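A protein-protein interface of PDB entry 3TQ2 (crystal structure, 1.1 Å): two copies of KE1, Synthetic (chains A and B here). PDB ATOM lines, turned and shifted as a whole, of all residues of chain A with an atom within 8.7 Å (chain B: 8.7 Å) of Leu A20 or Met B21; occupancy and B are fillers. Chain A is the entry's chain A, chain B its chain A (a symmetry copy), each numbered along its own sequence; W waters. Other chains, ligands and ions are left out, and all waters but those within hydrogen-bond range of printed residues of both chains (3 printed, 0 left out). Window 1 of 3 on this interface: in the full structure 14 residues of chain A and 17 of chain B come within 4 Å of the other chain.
The side-chain hydroxyl (OG) of Ser B25 sits at hydrogen-bond distance from the side-chain amino group (NZ) of Lys A23, 3.1 Å away.
O of Met B21 lies close to OG of Ser B25.
Among the printed residues, pairs that only touch across the chains: Leu A13 with Lys B14, Gln A16 with Phe B17, Leu A20 with Leu B20, Leu A20 with Met B21, Leu A20 with Val B24, Lys A23 with Lys B28, Val A24 with Val B24, Leu A27 with Leu B27 and Leu A27 with Lys B28.
Of chain B, only Leu B20, Met B21 and Val B24 come within 4 Å of Leu A20. Of chain A, only Leu A20 comes within 4 Å of Met B21. Of the printed residues of chain B, Lys A23 touches Ser B25 and Lys B28. Printed residues of chain A within 4 Å of Ser B25: Lys A23. Printed residues of chain A within 4 Å of Lys B14: Leu A13 (3.5 Å). Of the printed residues of chain A, Lys B28 touches Lys A23 (3.7 Å) and Leu A27 (3.8 Å). The nearest residue of chain B that does not touch Leu A20 is Phe B17 (4.1 Å). The nearest residue of chain A that does not touch Met B21 is Lys A23 (5.4 Å). The nearest printed residue of chain B that does not touch Leu A13 is Phe B17 (4.1 Å).
Printed residues of chain B that touch a printed residue of chain A: Lys B14, Phe B17, Leu B20, Met B21, Val B24, Ser B25, Leu B27 and Lys B28. Hydrophobic or aromatic side chains of chain A within 4 Å of the printed part of chain B: Leu A13, Leu A20, Val A24 and Leu A27.
Leu B20 touches its own counterpart, Leu A20. Leu A20 touches Val B24, but with the chains exchanged Val A24 does not touch Leu B20 (6.2 Å). Lys A23 touches Ser B25, but with the chains exchanged Ser A25 does not touch Lys B23 (11.9 Å). Leu A27 touches its own counterpart, Leu B27. Of the 10 pairs that touch across the chains among the printed residues, 3 have their exchanged pair printed and touching as well.
Water W1 lies within hydrogen-bond range of NZ of Lys A23 (2.7 Å) and OG of Ser B25 (3.3 Å). Water W3 lies within hydrogen-bond range of the side-chain sulfur of Met B21 (2.8 Å) and the side-chain amino group of Lys A23 (3.3 Å). Water W2 lies within hydrogen-bond range of O of Met B21 (3.0 Å), NZ of Lys A23 (3.0 Å) and OG of Ser B25 (3.1 Å).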
ATOM      1  N   LEU A  13     -25.062  25.219   6.902  1.00  0.00           N
ATOM      2  CA  LEU A  13     -24.130  24.609   7.848  1.00  0.00           C
ATOM      3  C   LEU A  13     -24.808  24.350   9.174  1.00  0.00           C
ATOM      4  O   LEU A  13     -24.530  23.345   9.827  1.00  0.00           O
ATOM      5  CB  LEU A  13     -22.932  25.529   7.962  1.00  0.00           C
ATOM      6  CG  LEU A  13     -21.705  24.976   8.689  1.00  0.00           C
ATOM      7  CD1 LEU A  13     -21.205  23.750   7.960  1.00  0.00           C
ATOM      8  CD2 LEU A  13     -20.671  26.079   8.888  1.00  0.00           C
ATOM      9  N   LYS A  14     -25.694  25.189   9.685  1.00  0.00           N
ATOM     10  CA  LYS A  14     -26.404  24.813  10.903  1.00  0.00           C
ATOM     11  C   LYS A  14     -27.241  23.546  10.758  1.00  0.00           C
ATOM     12  O   LYS A  14     -27.367  22.726  11.687  1.00  0.00           O
ATOM     13  CB  LYS A  14     -27.353  25.964  11.286  1.00  0.00           C
ATOM     14  CG  LYS A  14     -26.818  27.004  12.237  1.00  0.00           C
ATOM     15  CD  LYS A  14     -26.416  28.303  11.545  1.00  0.00           C
ATOM     16  CE  LYS A  14     -25.984  29.342  12.579  1.00  0.00           C
ATOM     17  NZ  LYS A  14     -24.502  29.517  12.589  1.00  0.00           N
ATOM     18  N   GLU A  15     -27.847  23.301   9.608  1.00  0.00           N
ATOM     19  CA  GLU A  15     -28.639  22.100   9.316  1.00  0.00           C
ATOM     20  C   GLU A  15     -27.688  20.909   9.268  1.00  0.00           C
ATOM     21  O   GLU A  15     -28.077  19.917   9.910  1.00  0.00           O
ATOM     22  CB  GLU A  15     -29.401  22.327   8.007  1.00  0.00           C
ATOM     23  CG  GLU A  15     -30.719  23.047   8.228  1.00  0.00           C
ATOM     24  CD  GLU A  15     -31.555  23.273   6.990  1.00  0.00           C
ATOM     25  OE1 GLU A  15     -31.650  24.437   6.534  1.00  0.00           O
ATOM     26  OE2 GLU A  15     -32.143  22.291   6.477  1.00  0.00           O
ATOM     27  N   GLN A  16     -26.556  21.042   8.624  1.00  0.00           N
ATOM     28  CA  GLN A  16     -25.513  20.003   8.614  1.00  0.00           C
ATOM     29  C   GLN A  16     -25.136  19.652  10.055  1.00  0.00           C
ATOM     30  O   GLN A  16     -25.030  18.419  10.305  1.00  0.00           O
ATOM     31  CB  GLN A  16     -24.280  20.363   7.788  1.00  0.00           C
ATOM     32  CG  GLN A  16     -24.586  20.732   6.338  1.00  0.00           C
ATOM     33  CD  GLN A  16     -23.284  21.127   5.639  1.00  0.00           C
ATOM     34  OE1 GLN A  16     -22.620  22.100   6.011  1.00  0.00           O
ATOM     35  NE2 GLN A  16     -22.851  20.352   4.646  1.00  0.00           N
ATOM     36  N   PHE A  17     -24.883  20.628  10.918  1.00  0.00           N
ATOM     37  CA  PHE A  17     -24.471  20.369  12.304  1.00  0.00           C
ATOM     38  C   PHE A  17     -25.539  19.583  13.041  1.00  0.00           C
ATOM     39  O   PHE A  17     -25.140  18.674  13.800  1.00  0.00           O
ATOM     40  CB  PHE A  17     -24.206  21.656  13.085  1.00  0.00           C
ATOM     41  CG  PHE A  17     -24.151  21.561  14.603  1.00  0.00           C
ATOM     42  CD1 PHE A  17     -23.072  21.000  15.273  1.00  0.00           C
ATOM     43  CD2 PHE A  17     -25.174  22.012  15.400  1.00  0.00           C
ATOM     44  CE1 PHE A  17     -23.054  20.912  16.652  1.00  0.00           C
ATOM     45  CE2 PHE A  17     -25.172  21.943  16.774  1.00  0.00           C
ATOM     46  CZ  PHE A  17     -24.090  21.381  17.431  1.00  0.00           C
ATOM     47  N   LEU A  18     -26.790  19.959  12.926  1.00  0.00           N
ATOM     48  CA  LEU A  18     -27.871  19.238  13.583  1.00  0.00           C
ATOM     49  C   LEU A  18     -27.863  17.785  13.111  1.00  0.00           C
ATOM     50  O   LEU A  18     -28.034  16.917  13.989  1.00  0.00           O
ATOM     51  CB  LEU A  18     -29.204  19.892  13.314  1.00  0.00           C
ATOM     52  CG  LEU A  18     -29.599  21.113  14.121  1.00  0.00           C
ATOM     53  CD1 LEU A  18     -30.999  21.538  13.714  1.00  0.00           C
ATOM     54  CD2 LEU A  18     -29.478  20.868  15.617  1.00  0.00           C
ATOM     55  N   MET A  19     -27.699  17.556  11.836  1.00  0.00           N
ATOM     56  CA  MET A  19     -27.697  16.149  11.395  1.00  0.00           C
ATOM     57  C   MET A  19     -26.480  15.367  11.943  1.00  0.00           C
ATOM     58  O   MET A  19     -26.634  14.209  12.343  1.00  0.00           O
ATOM     59  CB  MET A  19     -27.933  15.992   9.902  1.00  0.00           C
ATOM     60  CG  MET A  19     -29.491  16.087   9.535  1.00  0.00           C
ATOM     61  SD  MET A  19     -29.795  16.211   7.629  1.00  0.00           S
ATOM     62  CE  MET A  19     -28.181  16.565   6.962  1.00  0.00           C
ATOM     63  N   LEU A  20     -25.319  16.002  12.045  1.00  0.00           N
ATOM     64  CA  LEU A  20     -24.124  15.331  12.588  1.00  0.00           C
ATOM     65  C   LEU A  20     -24.279  15.137  14.086  1.00  0.00           C
ATOM     66  O   LEU A  20     -23.880  14.045  14.576  1.00  0.00           O
ATOM     67  CB  LEU A  20     -22.856  16.060  12.123  1.00  0.00           C
ATOM     68  CG  LEU A  20     -21.499  15.373  12.368  1.00  0.00           C
ATOM     69  CD1 LEU A  20     -21.435  14.087  11.569  1.00  0.00           C
ATOM     70  CD2 LEU A  20     -20.325  16.286  12.051  1.00  0.00           C
ATOM     71  N   MET A  21     -24.840  16.074  14.864  1.00  0.00           N
ATOM     72  CA  MET A  21     -25.165  15.844  16.254  1.00  0.00           C
ATOM     73  C   MET A  21     -26.081  14.647  16.399  1.00  0.00           C
ATOM     74  O   MET A  21     -25.885  13.817  17.316  1.00  0.00           O
ATOM     75  CB  MET A  21     -25.907  17.070  16.826  1.00  0.00           C
ATOM     76  CG  MET A  21     -24.949  18.239  16.990  1.00  0.00           C
ATOM     77  SD  MET A  21     -24.162  18.157  18.596  1.00  0.00           S
ATOM     78  CE  MET A  21     -25.161  19.198  19.641  1.00  0.00           C
ATOM     79  N   PHE A  22     -27.090  14.481  15.554  1.00  0.00           N
ATOM     80  CA  PHE A  22     -27.934  13.304  15.678  1.00  0.00           C
ATOM     81  C   PHE A  22     -27.108  12.038  15.410  1.00  0.00           C
ATOM     82  O   PHE A  22     -27.363  11.070  16.151  1.00  0.00           O
ATOM     83  CB  PHE A  22     -29.157  13.322  14.739  1.00  0.00           C
ATOM     84  CG  PHE A  22     -29.562  11.955  14.228  1.00  0.00           C
ATOM     85  CD1 PHE A  22     -30.208  11.034  15.008  1.00  0.00           C
ATOM     86  CD2 PHE A  22     -29.239  11.578  12.943  1.00  0.00           C
ATOM     87  CE1 PHE A  22     -30.496   9.756  14.591  1.00  0.00           C
ATOM     88  CE2 PHE A  22     -29.544  10.320  12.482  1.00  0.00           C
ATOM     89  CZ  PHE A  22     -30.189   9.420  13.301  1.00  0.00           C
ATOM     90  N   LYS A  23     -26.299  12.089  14.442  1.00  0.00           N
ATOM     91  CA  LYS A  23     -25.549  10.888  14.030  1.00  0.00           C
ATOM     92  C   LYS A  23     -24.608  10.510  15.158  1.00  0.00           C
ATOM     93  O   LYS A  23     -24.475   9.299  15.526  1.00  0.00           O
ATOM     94  CB  LYS A  23     -24.821  11.155  12.707  1.00  0.00           C
ATOM     95  CG  LYS A  23     -24.069   9.994  12.072  1.00  0.00           C
ATOM     96  CD  LYS A  23     -23.538  10.259  10.670  1.00  0.00           C
ATOM     97  CE  LYS A  23     -22.766   9.127  10.014  1.00  0.00           C
ATOM     98  NZ  LYS A  23     -22.397   9.279   8.577  1.00  0.00           N
ATOM     99  N   VAL A  24     -23.902  11.418  15.754  1.00  0.00           N
ATOM    100  CA  VAL A  24     -22.973  11.194  16.867  1.00  0.00           C
ATOM    101  C   VAL A  24     -23.753  10.773  18.097  1.00  0.00           C
ATOM    102  O   VAL A  24     -23.271   9.807  18.786  1.00  0.00           O
ATOM    103  CB  VAL A  24     -22.126  12.449  17.162  1.00  0.00           C
ATOM    104  CG1 VAL A  24     -21.221  12.286  18.369  1.00  0.00           C
ATOM    105  CG2 VAL A  24     -21.187  12.757  15.997  1.00  0.00           C
ATOM    106  N   SER A  25     -24.866  11.381  18.476  1.00  0.00           N
ATOM    107  CA  SER A  25     -25.611  10.854  19.636  1.00  0.00           C
ATOM    108  C   SER A  25     -26.066   9.413  19.423  1.00  0.00           C
ATOM    109  O   SER A  25     -25.992   8.605  20.388  1.00  0.00           O
ATOM    110  CB  SER A  25     -26.813  11.790  19.858  1.00  0.00           C
ATOM    111  OG  SER A  25     -26.386  12.927  20.591  1.00  0.00           O
ATOM    112  N   ALA A  26     -26.515   9.115  18.242  1.00  0.00           N
ATOM    113  CA  ALA A  26     -26.970   7.713  18.002  1.00  0.00           C
ATOM    114  C   ALA A  26     -25.778   6.771  18.113  1.00  0.00           C
ATOM    115  O   ALA A  26     -25.903   5.665  18.737  1.00  0.00           O
ATOM    116  CB  ALA A  26     -27.682   7.572  16.663  1.00  0.00           C
ATOM    117  N   LEU A  27     -24.618   7.157  17.613  1.00  0.00           N
ATOM    118  CA  LEU A  27     -23.401   6.314  17.690  1.00  0.00           C
ATOM    119  C   LEU A  27     -22.949   6.158  19.131  1.00  0.00           C
ATOM    120  O   LEU A  27     -22.544   4.992  19.545  1.00  0.00           O
ATOM    121  CB  LEU A  27     -22.262   6.880  16.834  1.00  0.00           C
ATOM    122  CG  LEU A  27     -21.051   5.953  16.572  1.00  0.00           C
ATOM    123  CD1 LEU A  27     -21.427   4.611  15.984  1.00  0.00           C
ATOM    124  CD2 LEU A  27     -20.048   6.631  15.627  1.00  0.00           C
ATOM    125  N   LYS B  14     -16.526  25.371   7.356  1.00  0.00           N
ATOM    126  CA  LYS B  14     -16.967  24.319   6.447  1.00  0.00           C
ATOM    127  C   LYS B  14     -15.929  23.222   6.229  1.00  0.00           C
ATOM    128  O   LYS B  14     -16.250  22.027   6.086  1.00  0.00           O
ATOM    129  CB  LYS B  14     -17.274  24.957   5.080  1.00  0.00           C
ATOM    130  CG  LYS B  14     -18.695  25.398   4.834  1.00  0.00           C
ATOM    131  CD  LYS B  14     -18.889  26.905   4.960  1.00  0.00           C
ATOM    132  CE  LYS B  14     -20.323  27.288   4.596  1.00  0.00           C
ATOM    133  NZ  LYS B  14     -21.122  27.624   5.810  1.00  0.00           N
ATOM    134  N   GLU B  15     -14.647  23.545   6.199  1.00  0.00           N
ATOM    135  CA  GLU B  15     -13.545  22.587   6.048  1.00  0.00           C
ATOM    136  C   GLU B  15     -13.480  21.739   7.314  1.00  0.00           C
ATOM    137  O   GLU B  15     -13.381  20.517   7.107  1.00  0.00           O
ATOM    138  CB  GLU B  15     -12.257  23.369   5.771  1.00  0.00           C
ATOM    139  CG  GLU B  15     -12.083  23.683   4.296  1.00  0.00           C
ATOM    140  CD  GLU B  15     -10.814  24.417   3.929  1.00  0.00           C
ATOM    141  OE1 GLU B  15     -10.892  25.621   3.592  1.00  0.00           O
ATOM    142  OE2 GLU B  15      -9.730  23.786   3.954  1.00  0.00           O
ATOM    143  N   GLN B  16     -13.587  22.340   8.472  1.00  0.00           N
ATOM    144  CA  GLN B  16     -13.661  21.611   9.749  1.00  0.00           C
ATOM    145  C   GLN B  16     -14.812  20.605   9.691  1.00  0.00           C
ATOM    146  O   GLN B  16     -14.550  19.453  10.137  1.00  0.00           O
ATOM    147  CB  GLN B  16     -13.768  22.512  10.978  1.00  0.00           C
ATOM    148  CG  GLN B  16     -12.653  23.548  11.093  1.00  0.00           C
ATOM    149  CD  GLN B  16     -12.907  24.419  12.323  1.00  0.00           C
ATOM    150  OE1 GLN B  16     -13.916  25.126  12.418  1.00  0.00           O
ATOM    151  NE2 GLN B  16     -12.032  24.351  13.327  1.00  0.00           N
ATOM    152  N   PHE B  17     -16.002  21.001   9.255  1.00  0.00           N
ATOM    153  CA  PHE B  17     -17.165  20.106   9.215  1.00  0.00           C
ATOM    154  C   PHE B  17     -16.894  18.917   8.313  1.00  0.00           C
ATOM    155  O   PHE B  17     -17.300  17.806   8.716  1.00  0.00           O
ATOM    156  CB  PHE B  17     -18.425  20.808   8.707  1.00  0.00           C
ATOM    157  CG  PHE B  17     -19.585  19.933   8.253  1.00  0.00           C
ATOM    158  CD1 PHE B  17     -20.396  19.251   9.150  1.00  0.00           C
ATOM    159  CD2 PHE B  17     -19.888  19.756   6.925  1.00  0.00           C
ATOM    160  CE1 PHE B  17     -21.432  18.451   8.710  1.00  0.00           C
ATOM    161  CE2 PHE B  17     -20.922  18.972   6.467  1.00  0.00           C
ATOM    162  CZ  PHE B  17     -21.724  18.296   7.371  1.00  0.00           C
ATOM    163  N   LEU B  18     -16.352  19.128   7.138  1.00  0.00           N
ATOM    164  CA  LEU B  18     -16.038  18.033   6.230  1.00  0.00           C
ATOM    165  C   LEU B  18     -15.082  17.066   6.924  1.00  0.00           C
ATOM    166  O   LEU B  18     -15.321  15.851   6.777  1.00  0.00           O
ATOM    167  CB  LEU B  18     -15.452  18.549   4.939  1.00  0.00           C
ATOM    168  CG  LEU B  18     -16.383  19.094   3.876  1.00  0.00           C
ATOM    169  CD1 LEU B  18     -15.564  19.482   2.657  1.00  0.00           C
ATOM    170  CD2 LEU B  18     -17.497  18.115   3.539  1.00  0.00           C
ATOM    171  N   MET B  19     -14.083  17.569   7.598  1.00  0.00           N
ATOM    172  CA  MET B  19     -13.166  16.622   8.260  1.00  0.00           C
ATOM    173  C   MET B  19     -13.860  15.837   9.398  1.00  0.00           C
ATOM    174  O   MET B  19     -13.619  14.634   9.538  1.00  0.00           O
ATOM    175  CB  MET B  19     -11.835  17.248   8.639  1.00  0.00           C
ATOM    176  CG  MET B  19     -10.835  17.316   7.389  1.00  0.00           C
ATOM    177  SD  MET B  19      -9.266  18.387   7.755  1.00  0.00           S
ATOM    178  CE  MET B  19      -9.680  19.249   9.258  1.00  0.00           C
ATOM    179  N   LEU B  20     -14.762  16.469  10.138  1.00  0.00           N
ATOM    180  CA  LEU B  20     -15.487  15.776  11.219  1.00  0.00           C
ATOM    181  C   LEU B  20     -16.489  14.801  10.625  1.00  0.00           C
ATOM    182  O   LEU B  20     -16.612  13.679  11.189  1.00  0.00           O
ATOM    183  CB  LEU B  20     -16.043  16.800  12.218  1.00  0.00           C
ATOM    184  CG  LEU B  20     -16.609  16.273  13.551  1.00  0.00           C
ATOM    185  CD1 LEU B  20     -15.496  15.625  14.349  1.00  0.00           C
ATOM    186  CD2 LEU B  20     -17.309  17.362  14.351  1.00  0.00           C
ATOM    187  N   MET B  21     -17.201  15.102   9.531  1.00  0.00           N
ATOM    188  CA  MET B  21     -18.023  14.132   8.841  1.00  0.00           C
ATOM    189  C   MET B  21     -17.198  12.930   8.427  1.00  0.00           C
ATOM    190  O   MET B  21     -17.661  11.776   8.569  1.00  0.00           O
ATOM    191  CB  MET B  21     -18.606  14.761   7.559  1.00  0.00           C
ATOM    192  CG  MET B  21     -19.678  15.780   7.909  1.00  0.00           C
ATOM    193  SD  MET B  21     -21.266  14.967   8.053  1.00  0.00           S
ATOM    194  CE  MET B  21     -22.015  15.157   6.446  1.00  0.00           C
ATOM    195  N   PHE B  22     -15.988  13.105   7.913  1.00  0.00           N
ATOM    196  CA  PHE B  22     -15.191  11.941   7.562  1.00  0.00           C
ATOM    197  C   PHE B  22     -14.867  11.130   8.824  1.00  0.00           C
ATOM    198  O   PHE B  22     -14.918   9.893   8.688  1.00  0.00           O
ATOM    199  CB  PHE B  22     -13.880  12.291   6.830  1.00  0.00           C
ATOM    200  CG  PHE B  22     -12.728  11.361   7.150  1.00  0.00           C
ATOM    201  CD1 PHE B  22     -12.639  10.092   6.646  1.00  0.00           C
ATOM    202  CD2 PHE B  22     -11.738  11.766   8.018  1.00  0.00           C
ATOM    203  CE1 PHE B  22     -11.653   9.202   7.001  1.00  0.00           C
ATOM    204  CE2 PHE B  22     -10.718  10.915   8.368  1.00  0.00           C
ATOM    205  CZ  PHE B  22     -10.669   9.643   7.844  1.00  0.00           C
ATOM    206  N   LYS B  23     -14.533  11.790   9.846  1.00  0.00           N
ATOM    207  CA  LYS B  23     -14.087  11.100  11.070  1.00  0.00           C
ATOM    208  C   LYS B  23     -15.259  10.311  11.620  1.00  0.00           C
ATOM    209  O   LYS B  23     -15.111   9.118  12.039  1.00  0.00           O
ATOM    210  CB  LYS B  23     -13.527  12.119  12.071  1.00  0.00           C
ATOM    211  CG  LYS B  23     -12.927  11.580  13.361  1.00  0.00           C
ATOM    212  CD  LYS B  23     -12.210  12.612  14.220  1.00  0.00           C
ATOM    213  CE  LYS B  23     -11.615  12.111  15.524  1.00  0.00           C
ATOM    214  NZ  LYS B  23     -10.747  13.046  16.297  1.00  0.00           N
ATOM    215  N   VAL B  24     -16.434  10.851  11.695  1.00  0.00           N
ATOM    216  CA  VAL B  24     -17.653  10.197  12.184  1.00  0.00           C
ATOM    217  C   VAL B  24     -18.051   9.091  11.227  1.00  0.00           C
ATOM    218  O   VAL B  24     -18.421   7.980  11.746  1.00  0.00           O
ATOM    219  CB  VAL B  24     -18.807  11.205  12.363  1.00  0.00           C
ATOM    220  CG1 VAL B  24     -20.110  10.550  12.777  1.00  0.00           C
ATOM    221  CG2 VAL B  24     -18.490  12.203  13.476  1.00  0.00           C
ATOM    222  N   SER B  25     -18.052   9.254   9.913  1.00  0.00           N
ATOM    223  CA  SER B  25     -18.370   8.101   9.049  1.00  0.00           C
ATOM    224  C   SER B  25     -17.394   6.946   9.246  1.00  0.00           C
ATOM    225  O   SER B  25     -17.843   5.767   9.259  1.00  0.00           O
ATOM    226  CB  SER B  25     -18.342   8.610   7.596  1.00  0.00           C
ATOM    227  OG  SER B  25     -19.582   9.233   7.299  1.00  0.00           O
ATOM    228  N   ALA B  26     -16.142   7.260   9.383  1.00  0.00           N
ATOM    229  CA  ALA B  26     -15.161   6.151   9.577  1.00  0.00           C
ATOM    230  C   ALA B  26     -15.439   5.459  10.905  1.00  0.00           C
ATOM    231  O   ALA B  26     -15.406   4.185  10.972  1.00  0.00           O
ATOM    232  CB  ALA B  26     -13.723   6.646   9.484  1.00  0.00           C
ATOM    233  N   LEU B  27     -15.775   6.200  11.946  1.00  0.00           N
ATOM    234  CA  LEU B  27     -16.079   5.613  13.272  1.00  0.00           C
ATOM    235  C   LEU B  27     -17.346   4.781  13.210  1.00  0.00           C
ATOM    236  O   LEU B  27     -17.385   3.637  13.831  1.00  0.00           O
ATOM    237  CB  LEU B  27     -16.203   6.690  14.357  1.00  0.00           C
ATOM    238  CG  LEU B  27     -16.208   6.210  15.828  1.00  0.00           C
ATOM    239  CD1 LEU B  27     -15.022   5.346  16.191  1.00  0.00           C
ATOM    240  CD2 LEU B  27     -16.244   7.410  16.785  1.00  0.00           C
ATOM    241  N   LYS B  28     -18.355   5.213  12.520  1.00  0.00           N
ATOM    242  CA  LYS B  28     -19.617   4.480  12.364  1.00  0.00           C
ATOM    243  C   LYS B  28     -19.354   3.131  11.703  1.00  0.00           C
ATOM    244  O   LYS B  28     -19.917   2.067  12.092  1.00  0.00           O
ATOM    245  CB  LYS B  28     -20.595   5.332  11.525  1.00  0.00           C
ATOM    246  CG  LYS B  28     -21.964   4.624  11.460  1.00  0.00           C
ATOM    247  CD  LYS B  28     -23.003   5.571  10.858  1.00  0.00           C
ATOM    248  CE  LYS B  28     -24.419   5.061  10.762  1.00  0.00           C
ATOM    249  NZ  LYS B  28     -24.585   4.020   9.703  1.00  0.00           N
HETATM  250  O   HOH W   1     -21.952   6.962   7.276  1.00  0.00           O
HETATM  251  O   HOH W   2     -20.558  11.558   9.104  1.00  0.00           O
HETATM  252  O   HOH W   3     -22.486  12.504   7.838  1.00  0.00           O
